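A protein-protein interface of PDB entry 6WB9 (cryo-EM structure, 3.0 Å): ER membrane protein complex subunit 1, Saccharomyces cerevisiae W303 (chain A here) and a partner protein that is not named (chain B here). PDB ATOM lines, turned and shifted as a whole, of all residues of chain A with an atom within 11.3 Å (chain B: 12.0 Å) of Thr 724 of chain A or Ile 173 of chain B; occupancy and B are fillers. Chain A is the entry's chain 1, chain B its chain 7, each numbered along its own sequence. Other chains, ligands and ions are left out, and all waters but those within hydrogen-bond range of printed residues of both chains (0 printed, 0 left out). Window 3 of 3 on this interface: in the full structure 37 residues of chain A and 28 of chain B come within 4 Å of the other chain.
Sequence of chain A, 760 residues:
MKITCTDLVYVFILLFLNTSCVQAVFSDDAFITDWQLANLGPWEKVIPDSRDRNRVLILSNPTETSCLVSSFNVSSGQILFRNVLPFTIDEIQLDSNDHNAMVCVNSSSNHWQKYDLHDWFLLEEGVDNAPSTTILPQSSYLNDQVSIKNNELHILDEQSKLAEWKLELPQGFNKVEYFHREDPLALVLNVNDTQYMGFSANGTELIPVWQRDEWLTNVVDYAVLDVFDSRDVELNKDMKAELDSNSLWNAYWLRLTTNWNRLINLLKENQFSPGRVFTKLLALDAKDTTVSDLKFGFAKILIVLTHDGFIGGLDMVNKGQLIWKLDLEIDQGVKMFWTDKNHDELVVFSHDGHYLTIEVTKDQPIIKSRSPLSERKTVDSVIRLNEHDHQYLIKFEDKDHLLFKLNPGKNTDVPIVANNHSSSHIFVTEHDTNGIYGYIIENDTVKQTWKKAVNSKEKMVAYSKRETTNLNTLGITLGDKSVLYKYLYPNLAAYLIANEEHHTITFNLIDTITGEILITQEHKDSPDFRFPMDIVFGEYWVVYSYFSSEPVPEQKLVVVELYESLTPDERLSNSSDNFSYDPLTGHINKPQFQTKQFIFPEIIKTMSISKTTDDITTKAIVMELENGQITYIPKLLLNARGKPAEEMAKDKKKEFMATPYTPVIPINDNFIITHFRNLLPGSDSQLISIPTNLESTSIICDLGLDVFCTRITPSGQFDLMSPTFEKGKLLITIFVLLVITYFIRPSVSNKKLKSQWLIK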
ATOM      1  N   VAL A  25      -2.876  -3.174  17.483  1.00  0.00           N
ATOM      2  CA  VAL A  25      -3.324  -1.815  17.226  1.00  0.00           C
ATOM      3  C   VAL A  25      -4.237  -1.863  16.005  1.00  0.00           C
ATOM      4  O   VAL A  25      -4.788  -0.855  15.563  1.00  0.00           O
ATOM      5  CB  VAL A  25      -2.111  -0.868  17.039  1.00  0.00           C
ATOM      6  CG1 VAL A  25      -1.488  -1.041  15.663  1.00  0.00           C
ATOM      7  CG2 VAL A  25      -2.478   0.587  17.321  1.00  0.00           C
ATOM      8  N   PHE A  26      -4.436  -3.073  15.493  1.00  0.00           N
ATOM      9  CA  PHE A  26      -5.006  -3.272  14.171  1.00  0.00           C
ATOM     10  C   PHE A  26      -6.271  -4.115  14.148  1.00  0.00           C
ATOM     11  O   PHE A  26      -7.133  -3.866  13.303  1.00  0.00           O
ATOM     12  CB  PHE A  26      -3.963  -3.930  13.251  1.00  0.00           C
ATOM     13  CG  PHE A  26      -3.968  -3.408  11.844  1.00  0.00           C
ATOM     14  CD1 PHE A  26      -4.886  -2.453  11.440  1.00  0.00           C
ATOM     15  CD2 PHE A  26      -3.049  -3.881  10.922  1.00  0.00           C
ATOM     16  CE1 PHE A  26      -4.886  -1.978  10.146  1.00  0.00           C
ATOM     17  CE2 PHE A  26      -3.045  -3.409   9.626  1.00  0.00           C
ATOM     18  CZ  PHE A  26      -3.964  -2.457   9.240  1.00  0.00           C
ATOM     19  N   SER A  27      -6.407  -5.104  15.036  1.00  0.00           N
ATOM     20  CA  SER A  27      -7.479  -6.088  14.901  1.00  0.00           C
ATOM     21  C   SER A  27      -8.845  -5.508  15.243  1.00  0.00           C
ATOM     22  O   SER A  27      -9.855  -5.938  14.675  1.00  0.00           O
ATOM     23  CB  SER A  27      -7.190  -7.304  15.778  1.00  0.00           C
ATOM     24  OG  SER A  27      -8.166  -8.312  15.583  1.00  0.00           O
ATOM     25  N   ASP A  28      -8.904  -4.537  16.153  1.00  0.00           N
ATOM     26  CA  ASP A  28     -10.164  -3.863  16.438  1.00  0.00           C
ATOM     27  C   ASP A  28     -10.484  -2.767  15.433  1.00  0.00           C
ATOM     28  O   ASP A  28     -11.562  -2.172  15.514  1.00  0.00           O
ATOM     29  CB  ASP A  28     -10.150  -3.269  17.850  1.00  0.00           C
ATOM     30  CG  ASP A  28      -9.086  -2.206  18.028  1.00  0.00           C
ATOM     31  OD1 ASP A  28      -7.888  -2.545  17.965  1.00  0.00           O
ATOM     32  OD2 ASP A  28      -9.448  -1.028  18.228  1.00  0.00           O
ATOM     33  N   ASP A  29      -9.575  -2.486  14.497  1.00  0.00           N
ATOM     34  CA  ASP A  29      -9.772  -1.463  13.483  1.00  0.00           C
ATOM     35  C   ASP A  29      -9.967  -2.023  12.082  1.00  0.00           C
ATOM     36  O   ASP A  29     -10.246  -1.247  11.163  1.00  0.00           O
ATOM     37  CB  ASP A  29      -8.584  -0.493  13.471  1.00  0.00           C
ATOM     38  CG  ASP A  29      -8.606   0.470  14.637  1.00  0.00           C
ATOM     39  OD1 ASP A  29      -9.712   0.831  15.088  1.00  0.00           O
ATOM     40  OD2 ASP A  29      -7.519   0.872  15.098  1.00  0.00           O
ATOM     41  N   ALA A  30      -9.816  -3.332  11.893  1.00  0.00           N
ATOM     42  CA  ALA A  30     -10.003  -3.934  10.581  1.00  0.00           C
ATOM     43  C   ALA A  30     -11.467  -3.866  10.166  1.00  0.00           C
ATOM     44  O   ALA A  30     -12.359  -4.197  10.953  1.00  0.00           O
ATOM     45  CB  ALA A  30      -9.523  -5.382  10.590  1.00  0.00           C
ATOM     46  N   ILE A  32     -13.246  -1.335   9.949  1.00  0.00           N
ATOM     47  CA  ILE A  32     -13.968  -0.390  10.794  1.00  0.00           C
ATOM     48  C   ILE A  32     -13.415   1.010  10.570  1.00  0.00           C
ATOM     49  O   ILE A  32     -14.158   1.931  10.214  1.00  0.00           O
ATOM     50  CB  ILE A  32     -13.883  -0.792  12.278  1.00  0.00           C
ATOM     51  CG1 ILE A  32     -14.651  -2.093  12.521  1.00  0.00           C
ATOM     52  CG2 ILE A  32     -14.420   0.317  13.167  1.00  0.00           C
ATOM     53  CD1 ILE A  32     -14.440  -2.686  13.891  1.00  0.00           C
ATOM     54  N   ASN A 670       2.019  -5.673   9.466  1.00  0.00           N
ATOM     55  CA  ASN A 670       1.276  -4.723  10.282  1.00  0.00           C
ATOM     56  C   ASN A 670       1.079  -3.403   9.552  1.00  0.00           C
ATOM     57  O   ASN A 670       0.129  -2.670   9.844  1.00  0.00           O
ATOM     58  CB  ASN A 670       1.999  -4.487  11.607  1.00  0.00           C
ATOM     59  CG  ASN A 670       2.581  -5.757  12.188  1.00  0.00           C
ATOM     60  OD1 ASN A 670       2.088  -6.856  11.931  1.00  0.00           O
ATOM     61  ND2 ASN A 670       3.637  -5.612  12.981  1.00  0.00           N
ATOM     62  N   THR A 713      -1.341   6.038  11.242  1.00  0.00           N
ATOM     63  CA  THR A 713      -0.536   6.751  12.231  1.00  0.00           C
ATOM     64  C   THR A 713       0.899   6.285  12.049  1.00  0.00           C
ATOM     65  O   THR A 713       1.249   5.173  12.483  1.00  0.00           O
ATOM     66  CB  THR A 713      -1.008   6.467  13.655  1.00  0.00           C
ATOM     67  OG1 THR A 713      -0.871   5.069  13.931  1.00  0.00           O
ATOM     68  CG2 THR A 713      -2.459   6.866  13.837  1.00  0.00           C
ATOM     69  N   GLY A 716       2.724   6.210  15.436  1.00  0.00           N
ATOM     70  CA  GLY A 716       1.806   5.769  16.460  1.00  0.00           C
ATOM     71  C   GLY A 716       0.786   6.841  16.800  1.00  0.00           C
ATOM     72  O   GLY A 716       0.979   8.029  16.557  1.00  0.00           O
ATOM     73  N   GLN A 717      -0.333   6.402  17.365  1.00  0.00           N
ATOM     74  CA  GLN A 717      -1.394   7.334  17.736  1.00  0.00           C
ATOM     75  C   GLN A 717      -1.041   7.944  19.083  1.00  0.00           C
ATOM     76  O   GLN A 717      -1.430   7.447  20.139  1.00  0.00           O
ATOM     77  CB  GLN A 717      -2.745   6.633  17.773  1.00  0.00           C
ATOM     78  CG  GLN A 717      -3.913   7.593  17.755  1.00  0.00           C
ATOM     79  CD  GLN A 717      -5.216   6.917  17.402  1.00  0.00           C
ATOM     80  OE1 GLN A 717      -5.618   5.945  18.040  1.00  0.00           O
ATOM     81  NE2 GLN A 717      -5.884   7.424  16.374  1.00  0.00           N
ATOM     82  N   LEU A 720      -4.188  10.598  20.657  1.00  0.00           N
ATOM     83  CA  LEU A 720      -5.487  10.063  21.022  1.00  0.00           C
ATOM     84  C   LEU A 720      -5.295   8.881  21.959  1.00  0.00           C
ATOM     85  O   LEU A 720      -4.329   8.126  21.826  1.00  0.00           O
ATOM     86  CB  LEU A 720      -6.270   9.644  19.770  1.00  0.00           C
ATOM     87  CG  LEU A 720      -7.677   9.071  19.908  1.00  0.00           C
ATOM     88  CD1 LEU A 720      -8.533   9.989  20.749  1.00  0.00           C
ATOM     89  CD2 LEU A 720      -8.305   8.845  18.546  1.00  0.00           C
ATOM     90  N   MET A 721      -6.244   8.706  22.874  1.00  0.00           N
ATOM     91  CA  MET A 721      -6.224   7.607  23.830  1.00  0.00           C
ATOM     92  C   MET A 721      -6.577   6.313  23.110  1.00  0.00           C
ATOM     93  O   MET A 721      -7.534   6.267  22.337  1.00  0.00           O
ATOM     94  CB  MET A 721      -7.212   7.870  24.961  1.00  0.00           C
ATOM     95  CG  MET A 721      -7.208   6.808  26.046  1.00  0.00           C
ATOM     96  SD  MET A 721      -8.309   7.230  27.406  1.00  0.00           S
ATOM     97  CE  MET A 721      -7.314   8.435  28.281  1.00  0.00           C
ATOM     98  N   SER A 722      -5.819   5.256  23.385  1.00  0.00           N
ATOM     99  CA  SER A 722      -6.018   3.985  22.711  1.00  0.00           C
ATOM    100  C   SER A 722      -7.376   3.387  23.078  1.00  0.00           C
ATOM    101  O   SER A 722      -7.886   3.620  24.177  1.00  0.00           O
ATOM    102  CB  SER A 722      -4.902   3.012  23.084  1.00  0.00           C
ATOM    103  OG  SER A 722      -5.098   1.739  22.494  1.00  0.00           O
ATOM    104  N   PRO A 723      -8.003   2.649  22.152  1.00  0.00           N
ATOM    105  CA  PRO A 723      -9.254   1.954  22.503  1.00  0.00           C
ATOM    106  C   PRO A 723      -9.064   0.874  23.551  1.00  0.00           C
ATOM    107  O   PRO A 723      -9.935   0.691  24.412  1.00  0.00           O
ATOM    108  CB  PRO A 723      -9.716   1.372  21.160  1.00  0.00           C
ATOM    109  CG  PRO A 723      -9.076   2.241  20.134  1.00  0.00           C
ATOM    110  CD  PRO A 723      -7.743   2.613  20.703  1.00  0.00           C
ATOM    111  N   THR A 724      -7.950   0.152  23.506  1.00  0.00           N
ATOM    112  CA  THR A 724      -7.606  -0.798  24.562  1.00  0.00           C
ATOM    113  C   THR A 724      -6.644  -0.157  25.561  1.00  0.00           C
ATOM    114  O   THR A 724      -5.544  -0.650  25.816  1.00  0.00           O
ATOM    115  CB  THR A 724      -7.016  -2.070  23.965  1.00  0.00           C
ATOM    116  OG1 THR A 724      -5.692  -1.805  23.487  1.00  0.00           O
ATOM    117  CG2 THR A 724      -7.882  -2.564  22.814  1.00  0.00           C
ATOM    118  N   PHE A 725      -7.075   0.971  26.121  1.00  0.00           N
ATOM    119  CA  PHE A 725      -6.364   1.607  27.221  1.00  0.00           C
ATOM    120  C   PHE A 725      -6.883   1.030  28.530  1.00  0.00           C
ATOM    121  O   PHE A 725      -8.095   1.003  28.767  1.00  0.00           O
ATOM    122  CB  PHE A 725      -6.543   3.125  27.193  1.00  0.00           C
ATOM    123  CG  PHE A 725      -5.834   3.838  28.309  1.00  0.00           C
ATOM    124  CD1 PHE A 725      -4.451   3.926  28.326  1.00  0.00           C
ATOM    125  CD2 PHE A 725      -6.550   4.421  29.340  1.00  0.00           C
ATOM    126  CE1 PHE A 725      -3.799   4.581  29.354  1.00  0.00           C
ATOM    127  CE2 PHE A 725      -5.904   5.076  30.371  1.00  0.00           C
ATOM    128  CZ  PHE A 725      -4.527   5.157  30.377  1.00  0.00           C
ATOM    129  N   GLU A 726      -5.964   0.565  29.373  1.00  0.00           N
ATOM    130  CA  GLU A 726      -6.317  -0.186  30.577  1.00  0.00           C
ATOM    131  C   GLU A 726      -6.823   0.775  31.650  1.00  0.00           C
ATOM    132  O   GLU A 726      -6.123   1.126  32.601  1.00  0.00           O
ATOM    133  CB  GLU A 726      -5.120  -0.991  31.063  1.00  0.00           C
ATOM    134  CG  GLU A 726      -4.564  -1.955  30.025  1.00  0.00           C
ATOM    135  CD  GLU A 726      -3.211  -2.518  30.414  1.00  0.00           C
ATOM    136  OE1 GLU A 726      -2.610  -2.011  31.384  1.00  0.00           O
ATOM    137  OE2 GLU A 726      -2.746  -3.467  29.748  1.00  0.00           O
ATOM    138  N   LYS A 727      -8.079   1.208  31.486  1.00  0.00           N
ATOM    139  CA  LYS A 727      -8.729   2.009  32.519  1.00  0.00           C
ATOM    140  C   LYS A 727      -9.128   1.159  33.716  1.00  0.00           C
ATOM    141  O   LYS A 727      -9.140   1.653  34.851  1.00  0.00           O
ATOM    142  CB  LYS A 727      -9.966   2.706  31.955  1.00  0.00           C
ATOM    143  CG  LYS A 727      -9.684   3.866  31.028  1.00  0.00           C
ATOM    144  CD  LYS A 727     -10.980   4.531  30.598  1.00  0.00           C
ATOM    145  CE  LYS A 727     -10.721   5.776  29.772  1.00  0.00           C
ATOM    146  NZ  LYS A 727     -11.988   6.440  29.361  1.00  0.00           N
ATOM    147  N   GLY A 728      -9.463  -0.111  33.477  1.00  0.00           N
ATOM    148  CA  GLY A 728      -9.888  -0.979  34.564  1.00  0.00           C
ATOM    149  C   GLY A 728      -8.759  -1.301  35.523  1.00  0.00           C
ATOM    150  O   GLY A 728      -8.923  -1.209  36.740  1.00  0.00           O
ATOM    151  N   LYS A 729      -7.587  -1.654  34.984  1.00  0.00           N
ATOM    152  CA  LYS A 729      -6.423  -1.893  35.830  1.00  0.00           C
ATOM    153  C   LYS A 729      -5.928  -0.604  36.475  1.00  0.00           C
ATOM    154  O   LYS A 729      -5.370  -0.641  37.577  1.00  0.00           O
ATOM    155  CB  LYS A 729      -5.307  -2.542  35.014  1.00  0.00           C
ATOM    156  CG  LYS A 729      -5.747  -3.743  34.197  1.00  0.00           C
ATOM    157  CD  LYS A 729      -4.630  -4.227  33.287  1.00  0.00           C
ATOM    158  CE  LYS A 729      -5.091  -5.386  32.420  1.00  0.00           C
ATOM    159  NZ  LYS A 729      -6.253  -5.016  31.568  1.00  0.00           N
ATOM    160  N   LEU A 730      -6.162   0.537  35.821  1.00  0.00           N
ATOM    161  CA  LEU A 730      -5.831   1.838  36.395  1.00  0.00           C
ATOM    162  C   LEU A 730      -6.659   2.111  37.648  1.00  0.00           C
ATOM    163  O   LEU A 730      -6.112   2.429  38.715  1.00  0.00           O
ATOM    164  CB  LEU A 730      -6.059   2.919  35.334  1.00  0.00           C
ATOM    165  CG  LEU A 730      -5.886   4.418  35.573  1.00  0.00           C
ATOM    166  CD1 LEU A 730      -4.444   4.741  35.921  1.00  0.00           C
ATOM    167  CD2 LEU A 730      -6.354   5.209  34.372  1.00  0.00           C
ATOM    168  N   ALA B 168      -1.359 -13.063   8.421  1.00  0.00           N
ATOM    169  CA  ALA B 168      -1.692 -12.450   9.714  1.00  0.00           C
ATOM    170  C   ALA B 168      -1.444 -10.937   9.705  1.00  0.00           C
ATOM    171  O   ALA B 168      -0.536 -10.414  10.353  1.00  0.00           O
ATOM    172  CB  ALA B 168      -0.937 -13.130  10.865  1.00  0.00           C
ATOM    173  N   ARG B 169      -2.268 -10.253   8.909  1.00  0.00           N
ATOM    174  CA  ARG B 169      -2.187  -8.798   8.821  1.00  0.00           C
ATOM    175  C   ARG B 169      -2.606  -8.128  10.122  1.00  0.00           C
ATOM    176  O   ARG B 169      -1.999  -7.135  10.538  1.00  0.00           O
ATOM    177  CB  ARG B 169      -3.055  -8.299   7.670  1.00  0.00           C
ATOM    178  CG  ARG B 169      -2.283  -7.569   6.599  1.00  0.00           C
ATOM    179  CD  ARG B 169      -1.289  -8.488   5.928  1.00  0.00           C
ATOM    180  NE  ARG B 169      -1.687  -8.796   4.564  1.00  0.00           N
ATOM    181  CZ  ARG B 169      -2.507  -9.783   4.234  1.00  0.00           C
ATOM    182  NH1 ARG B 169      -3.019 -10.564   5.170  1.00  0.00           N
ATOM    183  NH2 ARG B 169      -2.819  -9.988   2.967  1.00  0.00           N
ATOM    184  N   ASN B 170      -3.636  -8.653  10.779  1.00  0.00           N
ATOM    185  CA  ASN B 170      -4.226  -7.983  11.930  1.00  0.00           C
ATOM    186  C   ASN B 170      -3.409  -8.233  13.191  1.00  0.00           C
ATOM    187  O   ASN B 170      -3.054  -9.373  13.500  1.00  0.00           O
ATOM    188  CB  ASN B 170      -5.664  -8.450  12.127  1.00  0.00           C
ATOM    189  CG  ASN B 170      -6.583  -7.964  11.030  1.00  0.00           C
ATOM    190  OD1 ASN B 170      -6.478  -6.825  10.580  1.00  0.00           O
ATOM    191  ND2 ASN B 170      -7.486  -8.828  10.587  1.00  0.00           N
ATOM    192  N   VAL B 171      -3.115  -7.157  13.915  1.00  0.00           N
ATOM    193  CA  VAL B 171      -2.395  -7.214  15.180  1.00  0.00           C
ATOM    194  C   VAL B 171      -3.410  -7.097  16.306  1.00  0.00           C
ATOM    195  O   VAL B 171      -4.136  -6.100  16.397  1.00  0.00           O
ATOM    196  CB  VAL B 171      -1.335  -6.106  15.275  1.00  0.00           C
ATOM    197  CG1 VAL B 171      -0.784  -6.011  16.685  1.00  0.00           C
ATOM    198  CG2 VAL B 171      -0.219  -6.372  14.298  1.00  0.00           C
ATOM    199  N   SER B 172      -3.464  -8.112  17.162  1.00  0.00           N
ATOM    200  CA  SER B 172      -4.373  -8.086  18.296  1.00  0.00           C
ATOM    201  C   SER B 172      -3.845  -7.154  19.378  1.00  0.00           C
ATOM    202  O   SER B 172      -2.648  -7.139  19.680  1.00  0.00           O
ATOM    203  CB  SER B 172      -4.559  -9.495  18.856  1.00  0.00           C
ATOM    204  OG  SER B 172      -4.908 -10.407  17.830  1.00  0.00           O
ATOM    205  N   ILE B 173      -4.744  -6.364  19.955  1.00  0.00           N
ATOM    206  CA  ILE B 173      -4.379  -5.455  21.032  1.00  0.00           C
ATOM    207  C   ILE B 173      -5.481  -5.429  22.085  1.00  0.00           C
ATOM    208  O   ILE B 173      -6.551  -6.008  21.892  1.00  0.00           O
ATOM    209  CB  ILE B 173      -4.097  -4.043  20.497  1.00  0.00           C
ATOM    210  CG1 ILE B 173      -3.369  -3.202  21.545  1.00  0.00           C
ATOM    211  CG2 ILE B 173      -5.389  -3.365  20.078  1.00  0.00           C
ATOM    212  CD1 ILE B 173      -3.012  -1.812  21.070  1.00  0.00           C
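N of Thr 724 of chain A sits close to OG of Ser 722 of chain A, 3.4 Å away.
Of chain B, only Ile 173 (3.3 Å) comes within 4 Å of Thr 724 of chain A. Ile 173 of chain B touches three residues of chain A. Of chain B, only Val 171 (3.4 Å) and Ile 173 (3.4 Å) come within 4 Å of Val 25 of chain A. Printed residues of chain B within 4 Å of Asp 28 of chain A: Ile 173. No residue of chain B comes within 4 Å of Pro 723 of chain A. No residue of chain B comes within 4 Å of Phe 725 of chain A. Glu 726 of chain A touches none of the printed residues of chain B. Ser 172 of chain B touches just one residue of chain A: Ser 27 (3.9 Å). Of the printed residues of chain A, Asn 170 of chain B touches Ala 30 (3.4 Å). Of the printed residues of chain B, Ala 30 of chain A touches Asn 170 (3.4 Å). The nearest residue of chain B that does not touch Thr 724 of chain A is Ser 172 of chain B (7.0 Å).
Of the 22 printed residues of chain A, 7 touch a printed residue of chain B. Printed residues of chain A that touch a printed residue of chain B: Val 25, Phe 26, Ser 27, Asp 28, Ala 30, Asn 670 and Thr 724. Of the 6 printed residues of chain B, 5 touch a printed residue of chain A. Hydrophobic or aromatic side chains of chain B within 4 Å of the printed part of chain A: Val 171 and Ile 173. Among the printed residues, 10 pairs touch across the chains.
N of Val 25 of chain A sits at hydrogen-bond distance from O of Val 171 of chain B, 3.4 Å away. O of Val 171 of chain B lies within hydrogen-bond range of N of Phe 26 of chain A (3.2 Å). The backbone carbonyl oxygen (O) of Val 171 of chain B sits at hydrogen-bond distance from the backbone NH (N) of Ser 27 of chain A, 2.8 Å away.
N of Val 25 of chain A touches CB of Ile 173 of chain B, 3.4 Å away. CD2 of Phe 26 of chain A touches O of Arg 169 of chain B, 3.4 Å away. Ser 172 of chain B touches Ser 27 of chain A (CA to CB, 3.9 Å). OD1 of Asp 28 of chain A touches CG2 of Ile 173 of chain B, 3.4 Å away. Ala 30 of chain A touches Asn 170 of chain B (CB to OD1, 3.4 Å). OD1 of Asn 670 of chain A touches CG2 of Val 171 of chain B (3.3 Å). CG1 of Ile 173 of chain B touches OG1 of Thr 724 of chain A, 3.3 Å away.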
